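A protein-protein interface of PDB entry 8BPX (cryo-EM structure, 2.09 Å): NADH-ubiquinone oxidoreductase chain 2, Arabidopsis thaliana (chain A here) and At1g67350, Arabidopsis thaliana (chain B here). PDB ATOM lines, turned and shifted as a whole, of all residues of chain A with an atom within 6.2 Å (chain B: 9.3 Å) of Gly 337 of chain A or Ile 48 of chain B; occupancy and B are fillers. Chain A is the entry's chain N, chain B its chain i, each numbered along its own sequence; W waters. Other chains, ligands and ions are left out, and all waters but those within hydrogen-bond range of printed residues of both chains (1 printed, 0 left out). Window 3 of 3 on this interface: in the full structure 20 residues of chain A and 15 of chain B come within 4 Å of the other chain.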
ATOM      1  N   ILE A 282      -0.175  31.547  12.974  1.00  0.00           N
ATOM      2  CA  ILE A 282      -1.647  31.315  13.003  1.00  0.00           C
ATOM      3  C   ILE A 282      -2.304  31.364  11.607  1.00  0.00           C
ATOM      4  O   ILE A 282      -3.078  30.418  11.338  1.00  0.00           O
ATOM      5  CB  ILE A 282      -2.232  32.362  14.004  1.00  0.00           C
ATOM      6  CG1 ILE A 282      -2.142  31.926  15.468  1.00  0.00           C
ATOM      7  CG2 ILE A 282      -3.630  32.800  13.603  1.00  0.00           C
ATOM      8  CD1 ILE A 282      -3.232  30.981  15.887  1.00  0.00           C
ATOM      9  N   GLN A 291       3.716  25.253  17.394  1.00  0.00           N
ATOM     10  CA  GLN A 291       3.010  25.350  18.661  1.00  0.00           C
ATOM     11  C   GLN A 291       3.784  24.648  19.767  1.00  0.00           C
ATOM     12  O   GLN A 291       3.776  25.106  20.912  1.00  0.00           O
ATOM     13  CB  GLN A 291       1.599  24.779  18.525  1.00  0.00           C
ATOM     14  CG  GLN A 291       0.668  25.680  17.725  1.00  0.00           C
ATOM     15  CD  GLN A 291      -0.606  24.978  17.311  1.00  0.00           C
ATOM     16  OE1 GLN A 291      -1.071  24.062  17.989  1.00  0.00           O
ATOM     17  NE2 GLN A 291      -1.180  25.403  16.192  1.00  0.00           N
ATOM     18  N   ILE A 332       1.387  30.523  26.256  1.00  0.00           N
ATOM     19  CA  ILE A 332       0.550  29.330  26.418  1.00  0.00           C
ATOM     20  C   ILE A 332      -0.711  29.434  25.559  1.00  0.00           C
ATOM     21  O   ILE A 332      -1.156  28.446  24.962  1.00  0.00           O
ATOM     22  CB  ILE A 332       0.215  29.094  27.903  1.00  0.00           C
ATOM     23  CG1 ILE A 332       1.398  28.420  28.590  1.00  0.00           C
ATOM     24  CG2 ILE A 332      -1.039  28.236  28.050  1.00  0.00           C
ATOM     25  CD1 ILE A 332       1.940  27.229  27.816  1.00  0.00           C
ATOM     26  N   GLY A 333      -1.282  30.636  25.452  1.00  0.00           N
ATOM     27  CA  GLY A 333      -2.474  30.812  24.636  1.00  0.00           C
ATOM     28  C   GLY A 333      -2.228  30.595  23.152  1.00  0.00           C
ATOM     29  O   GLY A 333      -3.039  29.966  22.467  1.00  0.00           O
ATOM     30  N   PHE A 334      -1.116  31.122  22.635  1.00  0.00           N
ATOM     31  CA  PHE A 334      -0.740  30.865  21.247  1.00  0.00           C
ATOM     32  C   PHE A 334      -0.538  29.375  21.005  1.00  0.00           C
ATOM     33  O   PHE A 334      -0.906  28.853  19.945  1.00  0.00           O
ATOM     34  CB  PHE A 334       0.536  31.641  20.906  1.00  0.00           C
ATOM     35  CG  PHE A 334       1.075  31.367  19.530  1.00  0.00           C
ATOM     36  CD1 PHE A 334       0.408  31.803  18.402  1.00  0.00           C
ATOM     37  CD2 PHE A 334       2.249  30.650  19.367  1.00  0.00           C
ATOM     38  CE1 PHE A 334       0.918  31.549  17.140  1.00  0.00           C
ATOM     39  CE2 PHE A 334       2.758  30.391  18.105  1.00  0.00           C
ATOM     40  CZ  PHE A 334       2.089  30.839  16.992  1.00  0.00           C
ATOM     41  N   SER A 335       0.035  28.673  21.985  1.00  0.00           N
ATOM     42  CA  SER A 335       0.368  27.264  21.803  1.00  0.00           C
ATOM     43  C   SER A 335      -0.871  26.402  21.570  1.00  0.00           C
ATOM     44  O   SER A 335      -0.854  25.500  20.726  1.00  0.00           O
ATOM     45  CB  SER A 335       1.149  26.756  23.017  1.00  0.00           C
ATOM     46  OG  SER A 335       1.468  25.384  22.887  1.00  0.00           O
ATOM     47  N   CYS A 336      -1.985  26.649  22.280  1.00  0.00           N
ATOM     48  CA  CYS A 336      -3.102  25.643  22.271  1.00  0.00           C
ATOM     49  C   CYS A 336      -3.920  25.806  20.970  1.00  0.00           C
ATOM     50  O   CYS A 336      -4.759  24.939  20.720  1.00  0.00           O
ATOM     51  CB  CYS A 336      -4.000  25.634  23.527  1.00  0.00           C
ATOM     52  SG  CYS A 336      -3.765  24.229  24.683  1.00  0.00           S
ATOM     53  N   GLY A 337      -3.672  26.852  20.165  1.00  0.00           N
ATOM     54  CA  GLY A 337      -4.217  26.900  18.820  1.00  0.00           C
ATOM     55  C   GLY A 337      -5.728  26.859  18.711  1.00  0.00           C
ATOM     56  O   GLY A 337      -6.267  26.094  17.908  1.00  0.00           O
ATOM     57  N   THR A 338      -6.427  27.667  19.506  1.00  0.00           N
ATOM     58  CA  THR A 338      -7.877  27.778  19.429  1.00  0.00           C
ATOM     59  C   THR A 338      -8.267  29.249  19.444  1.00  0.00           C
ATOM     60  O   THR A 338      -7.471  30.115  19.814  1.00  0.00           O
ATOM     61  CB  THR A 338      -8.580  27.044  20.584  1.00  0.00           C
ATOM     62  OG1 THR A 338      -8.300  27.708  21.823  1.00  0.00           O
ATOM     63  CG2 THR A 338      -8.131  25.597  20.671  1.00  0.00           C
ATOM     64  N   ILE A 339      -9.467  29.572  18.933  1.00  0.00           N
ATOM     65  CA  ILE A 339     -10.045  30.940  19.030  1.00  0.00           C
ATOM     66  C   ILE A 339      -9.944  31.466  20.492  1.00  0.00           C
ATOM     67  O   ILE A 339      -9.493  32.550  20.648  1.00  0.00           O
ATOM     68  CB  ILE A 339     -11.491  31.062  18.469  1.00  0.00           C
ATOM     69  CG1 ILE A 339     -11.547  30.861  16.960  1.00  0.00           C
ATOM     70  CG2 ILE A 339     -12.095  32.401  18.845  1.00  0.00           C
ATOM     71  CD1 ILE A 339     -10.680  31.809  16.193  1.00  0.00           C
ATOM     72  N   GLY A 341      -7.779  30.532  22.688  1.00  0.00           N
ATOM     73  CA  GLY A 341      -6.363  30.748  22.945  1.00  0.00           C
ATOM     74  C   GLY A 341      -5.889  32.114  22.484  1.00  0.00           C
ATOM     75  O   GLY A 341      -5.205  32.830  23.218  1.00  0.00           O
ATOM     76  N   ILE A 342      -6.257  32.482  21.265  1.00  0.00           N
ATOM     77  CA  ILE A 342      -5.895  33.807  20.687  1.00  0.00           C
ATOM     78  C   ILE A 342      -6.537  34.916  21.530  1.00  0.00           C
ATOM     79  O   ILE A 342      -5.814  35.767  21.967  1.00  0.00           O
ATOM     80  CB  ILE A 342      -6.204  33.945  19.175  1.00  0.00           C
ATOM     81  CG1 ILE A 342      -5.186  33.191  18.322  1.00  0.00           C
ATOM     82  CG2 ILE A 342      -6.243  35.400  18.766  1.00  0.00           C
ATOM     83  CD1 ILE A 342      -5.199  31.720  18.508  1.00  0.00           C
ATOM     84  N   TYR A 412      -6.839  31.779  32.649  1.00  0.00           N
ATOM     85  CA  TYR A 412      -6.691  31.152  31.309  1.00  0.00           C
ATOM     86  C   TYR A 412      -5.497  30.193  31.270  1.00  0.00           C
ATOM     87  O   TYR A 412      -5.641  29.121  30.673  1.00  0.00           O
ATOM     88  CB  TYR A 412      -6.538  32.138  30.153  1.00  0.00           C
ATOM     89  CG  TYR A 412      -6.305  31.358  28.883  1.00  0.00           C
ATOM     90  CD1 TYR A 412      -7.356  30.716  28.247  1.00  0.00           C
ATOM     91  CD2 TYR A 412      -5.027  31.153  28.386  1.00  0.00           C
ATOM     92  CE1 TYR A 412      -7.154  29.953  27.110  1.00  0.00           C
ATOM     93  CE2 TYR A 412      -4.805  30.377  27.261  1.00  0.00           C
ATOM     94  CZ  TYR A 412      -5.875  29.786  26.613  1.00  0.00           C
ATOM     95  OH  TYR A 412      -5.666  29.031  25.497  1.00  0.00           O
ATOM     96  N   TYR A 498      -8.989  35.138  10.562  1.00  0.00           N
ATOM     97  CA  TYR A 498      -9.372  34.132   9.518  1.00  0.00           C
ATOM     98  C   TYR A 498     -10.668  34.485   8.817  1.00  0.00           C
ATOM     99  O   TYR A 498     -11.129  33.676   8.089  1.00  0.00           O
ATOM    100  CB  TYR A 498      -9.675  32.821  10.214  1.00  0.00           C
ATOM    101  CG  TYR A 498      -8.786  32.536  11.388  1.00  0.00           C
ATOM    102  CD1 TYR A 498      -9.132  32.961  12.656  1.00  0.00           C
ATOM    103  CD2 TYR A 498      -7.575  31.892  11.215  1.00  0.00           C
ATOM    104  CE1 TYR A 498      -8.296  32.738  13.734  1.00  0.00           C
ATOM    105  CE2 TYR A 498      -6.737  31.650  12.283  1.00  0.00           C
ATOM    106  CZ  TYR A 498      -7.097  32.083  13.543  1.00  0.00           C
ATOM    107  OH  TYR A 498      -6.284  31.862  14.613  1.00  0.00           O
ATOM    108  N   MET B  43     -19.747  27.055  21.030  1.00  0.00           N
ATOM    109  CA  MET B  43     -18.746  28.035  20.620  1.00  0.00           C
ATOM    110  C   MET B  43     -17.335  27.530  20.890  1.00  0.00           C
ATOM    111  O   MET B  43     -16.419  27.779  20.099  1.00  0.00           O
ATOM    112  CB  MET B  43     -18.990  29.363  21.337  1.00  0.00           C
ATOM    113  CG  MET B  43     -18.755  30.595  20.477  1.00  0.00           C
ATOM    114  SD  MET B  43     -18.635  32.097  21.466  1.00  0.00           S
ATOM    115  CE  MET B  43     -20.364  32.520  21.656  1.00  0.00           C
ATOM    116  N   TRP B  44     -17.140  26.816  22.002  1.00  0.00           N
ATOM    117  CA  TRP B  44     -15.823  26.285  22.333  1.00  0.00           C
ATOM    118  C   TRP B  44     -15.365  25.215  21.349  1.00  0.00           C
ATOM    119  O   TRP B  44     -14.166  24.930  21.276  1.00  0.00           O
ATOM    120  CB  TRP B  44     -15.826  25.725  23.759  1.00  0.00           C
ATOM    121  CG  TRP B  44     -15.687  26.782  24.816  1.00  0.00           C
ATOM    122  CD1 TRP B  44     -15.226  28.053  24.642  1.00  0.00           C
ATOM    123  CD2 TRP B  44     -16.020  26.664  26.206  1.00  0.00           C
ATOM    124  NE1 TRP B  44     -15.246  28.732  25.835  1.00  0.00           N
ATOM    125  CE2 TRP B  44     -15.727  27.902  26.811  1.00  0.00           C
ATOM    126  CE3 TRP B  44     -16.530  25.629  26.996  1.00  0.00           C
ATOM    127  CZ2 TRP B  44     -15.934  28.136  28.167  1.00  0.00           C
ATOM    128  CZ3 TRP B  44     -16.733  25.862  28.343  1.00  0.00           C
ATOM    129  CH2 TRP B  44     -16.437  27.107  28.914  1.00  0.00           C
ATOM    130  N   ALA B  45     -16.287  24.620  20.595  1.00  0.00           N
ATOM    131  CA  ALA B  45     -15.949  23.633  19.579  1.00  0.00           C
ATOM    132  C   ALA B  45     -15.778  24.239  18.192  1.00  0.00           C
ATOM    133  O   ALA B  45     -15.503  23.500  17.242  1.00  0.00           O
ATOM    134  CB  ALA B  45     -17.020  22.538  19.531  1.00  0.00           C
ATOM    135  N   LEU B  46     -15.934  25.552  18.054  1.00  0.00           N
ATOM    136  CA  LEU B  46     -15.782  26.190  16.750  1.00  0.00           C
ATOM    137  C   LEU B  46     -14.334  26.079  16.287  1.00  0.00           C
ATOM    138  O   LEU B  46     -13.416  26.384  17.060  1.00  0.00           O
ATOM    139  CB  LEU B  46     -16.201  27.659  16.818  1.00  0.00           C
ATOM    140  CG  LEU B  46     -17.517  28.044  16.138  1.00  0.00           C
ATOM    141  CD1 LEU B  46     -17.927  29.453  16.530  1.00  0.00           C
ATOM    142  CD2 LEU B  46     -17.407  27.924  14.629  1.00  0.00           C
ATOM    143  N   PRO B  47     -14.085  25.642  15.055  1.00  0.00           N
ATOM    144  CA  PRO B  47     -12.700  25.497  14.592  1.00  0.00           C
ATOM    145  C   PRO B  47     -11.992  26.842  14.522  1.00  0.00           C
ATOM    146  O   PRO B  47     -12.552  27.837  14.055  1.00  0.00           O
ATOM    147  CB  PRO B  47     -12.858  24.866  13.204  1.00  0.00           C
ATOM    148  CG  PRO B  47     -14.217  25.289  12.764  1.00  0.00           C
ATOM    149  CD  PRO B  47     -15.051  25.262  14.011  1.00  0.00           C
ATOM    150  N   ILE B  48     -10.735  26.920  14.914  1.00  0.00           N
ATOM    151  CA  ILE B  48     -10.016  28.203  14.785  1.00  0.00           C
ATOM    152  C   ILE B  48      -9.638  28.370  13.306  1.00  0.00           C
ATOM    153  O   ILE B  48      -9.555  29.528  12.837  1.00  0.00           O
ATOM    154  CB  ILE B  48      -8.800  28.162  15.740  1.00  0.00           C
ATOM    155  CG1 ILE B  48      -7.965  29.439  15.750  1.00  0.00           C
ATOM    156  CG2 ILE B  48      -7.932  26.948  15.434  1.00  0.00           C
ATOM    157  CD1 ILE B  48      -6.653  29.258  16.463  1.00  0.00           C
ATOM    158  N   ARG B  49      -9.396  27.243  12.625  1.00  0.00           N
ATOM    159  CA  ARG B  49      -9.132  27.312  11.194  1.00  0.00           C
ATOM    160  C   ARG B  49     -10.396  26.892  10.461  1.00  0.00           C
ATOM    161  O   ARG B  49     -10.697  25.690  10.381  1.00  0.00           O
ATOM    162  CB  ARG B  49      -7.956  26.401  10.830  1.00  0.00           C
ATOM    163  CG  ARG B  49      -7.387  26.577   9.435  1.00  0.00           C
ATOM    164  CD  ARG B  49      -8.080  25.656   8.440  1.00  0.00           C
ATOM    165  NE  ARG B  49      -7.894  24.249   8.777  1.00  0.00           N
ATOM    166  CZ  ARG B  49      -8.450  23.243   8.117  1.00  0.00           C
ATOM    167  NH1 ARG B  49      -9.232  23.451   7.070  1.00  0.00           N
ATOM    168  NH2 ARG B  49      -8.214  21.996   8.516  1.00  0.00           N
ATOM    169  N   PRO B  50     -11.181  27.873   9.939  1.00  0.00           N
ATOM    170  CA  PRO B  50     -12.432  27.510   9.299  1.00  0.00           C
ATOM    171  C   PRO B  50     -12.228  26.619   8.064  1.00  0.00           C
ATOM    172  O   PRO B  50     -11.122  26.518   7.596  1.00  0.00           O
ATOM    173  CB  PRO B  50     -13.036  28.907   9.021  1.00  0.00           C
ATOM    174  CG  PRO B  50     -11.885  29.819   8.844  1.00  0.00           C
ATOM    175  CD  PRO B  50     -10.954  29.334   9.914  1.00  0.00           C
ATOM    176  N   TYR B  51     -13.270  25.981   7.589  1.00  0.00           N
ATOM    177  CA  TYR B  51     -13.236  25.164   6.385  1.00  0.00           C
ATOM    178  C   TYR B  51     -12.981  26.033   5.161  1.00  0.00           C
ATOM    179  O   TYR B  51     -13.801  26.892   4.818  1.00  0.00           O
ATOM    180  CB  TYR B  51     -14.559  24.415   6.242  1.00  0.00           C
ATOM    181  CG  TYR B  51     -14.529  23.220   5.317  1.00  0.00           C
ATOM    182  CD1 TYR B  51     -13.487  22.307   5.356  1.00  0.00           C
ATOM    183  CD2 TYR B  51     -15.554  23.004   4.407  1.00  0.00           C
ATOM    184  CE1 TYR B  51     -13.466  21.212   4.514  1.00  0.00           C
ATOM    185  CE2 TYR B  51     -15.544  21.915   3.565  1.00  0.00           C
ATOM    186  CZ  TYR B  51     -14.499  21.020   3.621  1.00  0.00           C
ATOM    187  OH  TYR B  51     -14.492  19.937   2.779  1.00  0.00           O
ATOM    188  N   PHE B  53     -10.662  28.466   4.474  1.00  0.00           N
ATOM    189  CA  PHE B  53     -10.552  29.900   4.720  1.00  0.00           C
ATOM    190  C   PHE B  53      -9.919  30.616   3.532  1.00  0.00           C
ATOM    191  O   PHE B  53     -10.316  31.734   3.190  1.00  0.00           O
ATOM    192  CB  PHE B  53      -9.754  30.163   5.996  1.00  0.00           C
ATOM    193  CG  PHE B  53      -8.342  29.655   5.951  1.00  0.00           C
ATOM    194  CD1 PHE B  53      -8.051  28.343   6.279  1.00  0.00           C
ATOM    195  CD2 PHE B  53      -7.302  30.492   5.586  1.00  0.00           C
ATOM    196  CE1 PHE B  53      -6.750  27.879   6.239  1.00  0.00           C
ATOM    197  CE2 PHE B  53      -6.003  30.030   5.544  1.00  0.00           C
ATOM    198  CZ  PHE B  53      -5.727  28.726   5.870  1.00  0.00           C
ATOM    199  N   PHE B  56     -12.094  32.384   1.058  1.00  0.00           N
ATOM    200  CA  PHE B  56     -12.740  33.659   1.421  1.00  0.00           C
ATOM    201  C   PHE B  56     -12.128  34.817   0.599  1.00  0.00           C
ATOM    202  O   PHE B  56     -10.891  34.870   0.480  1.00  0.00           O
ATOM    203  CB  PHE B  56     -12.699  33.842   2.931  1.00  0.00           C
ATOM    204  CG  PHE B  56     -13.230  32.741   3.811  1.00  0.00           C
ATOM    205  CD1 PHE B  56     -14.129  31.800   3.342  1.00  0.00           C
ATOM    206  CD2 PHE B  56     -12.817  32.651   5.130  1.00  0.00           C
ATOM    207  CE1 PHE B  56     -14.591  30.788   4.166  1.00  0.00           C
ATOM    208  CE2 PHE B  56     -13.270  31.629   5.952  1.00  0.00           C
ATOM    209  CZ  PHE B  56     -14.161  30.706   5.466  1.00  0.00           C
ATOM    210  N   HIS B  59      -8.852  36.598   0.877  1.00  0.00           N
ATOM    211  CA  HIS B  59      -7.594  35.866   0.663  1.00  0.00           C
ATOM    212  C   HIS B  59      -7.265  35.668  -0.833  1.00  0.00           C
ATOM    213  O   HIS B  59      -6.233  35.121  -1.141  1.00  0.00           O
ATOM    214  CB  HIS B  59      -7.723  34.592   1.439  1.00  0.00           C
ATOM    215  CG  HIS B  59      -8.135  34.712   2.874  1.00  0.00           C
ATOM    216  ND1 HIS B  59      -8.251  33.612   3.685  1.00  0.00           N
ATOM    217  CD2 HIS B  59      -8.476  35.770   3.639  1.00  0.00           C
ATOM    218  CE1 HIS B  59      -8.644  33.981   4.883  1.00  0.00           C
ATOM    219  NE2 HIS B  59      -8.795  35.300   4.880  1.00  0.00           N
HETATM  220  O   HOH W   1     -11.256  27.684  19.018  1.00  0.00           O
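Printed residues of chain B that touch a printed residue of chain A: Ile 48, Pro 50 and Phe 56. Of the 14 printed residues of chain A, 6 touch a printed residue of chain B. Hydrophobic or aromatic side chains of chain A that line the printed part of chain B: Ile 282, Ile 339, Ile 342 and Tyr 498. Among the printed residues, 8 pairs touch across the chains.
Of the printed residues of chain B, Ile 282 of chain A touches Ile 48. No residue of chain B comes within 4 Å of Cys 336 of chain A. Of the printed residues of chain B, Gly 337 of chain A touches Ile 48. Thr 338 of chain A touches just one residue of chain B: Ile 48 (3.4 Å). Of the printed residues of chain B, Ile 339 of chain A touches Ile 48 (3.5 Å). Printed residues of chain B within 4 Å of Tyr 498 of chain A: Ile 48, Pro 50 and Phe 56. Pro 47 of chain B touches none of the printed residues of chain A. Of chain A, only Ile 282, Gly 337, Thr 338, Ile 339, Ile 342 and Tyr 498 come within 4 Å of Ile 48 of chain B. Printed residues of chain A within 4 Å of Pro 50 of chain B: Tyr 498. Printed residues of chain A within 4 Å of Phe 56 of chain B: Tyr 498 (3.6 Å).
Water W1 lies within hydrogen-bond range of N of Ile 339 of chain A (2.6 Å) and O of Leu 46 of chain B (3.2 Å).
The backbone NH of Gly 341 of chain A sits at hydrogen-bond distance from the side-chain hydroxyl of Thr 338 of chain A (3.0 Å).
Ile 282 of chain A touches Ile 48 of chain B (CD1 to CD1, 3.9 Å). Ile 48 of chain B touches Gly 337 of chain A. Ile 48 of chain B touches Thr 338 of chain A. N of Ile 339 of chain A touches CG1 of Ile 48 of chain B, 3.5 Å away. Ile 48 of chain B touches Ile 342 of chain A (CD1 to CD1, 3.5 Å). OH of Tyr 498 of chain A touches CG1 of Ile 48 of chain B, 3.2 Å away. Tyr 498 of chain A touches Pro 50 of chain B. Tyr 498 of chain A touches Phe 56 of chain B (O to CD2, 3.6 Å).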
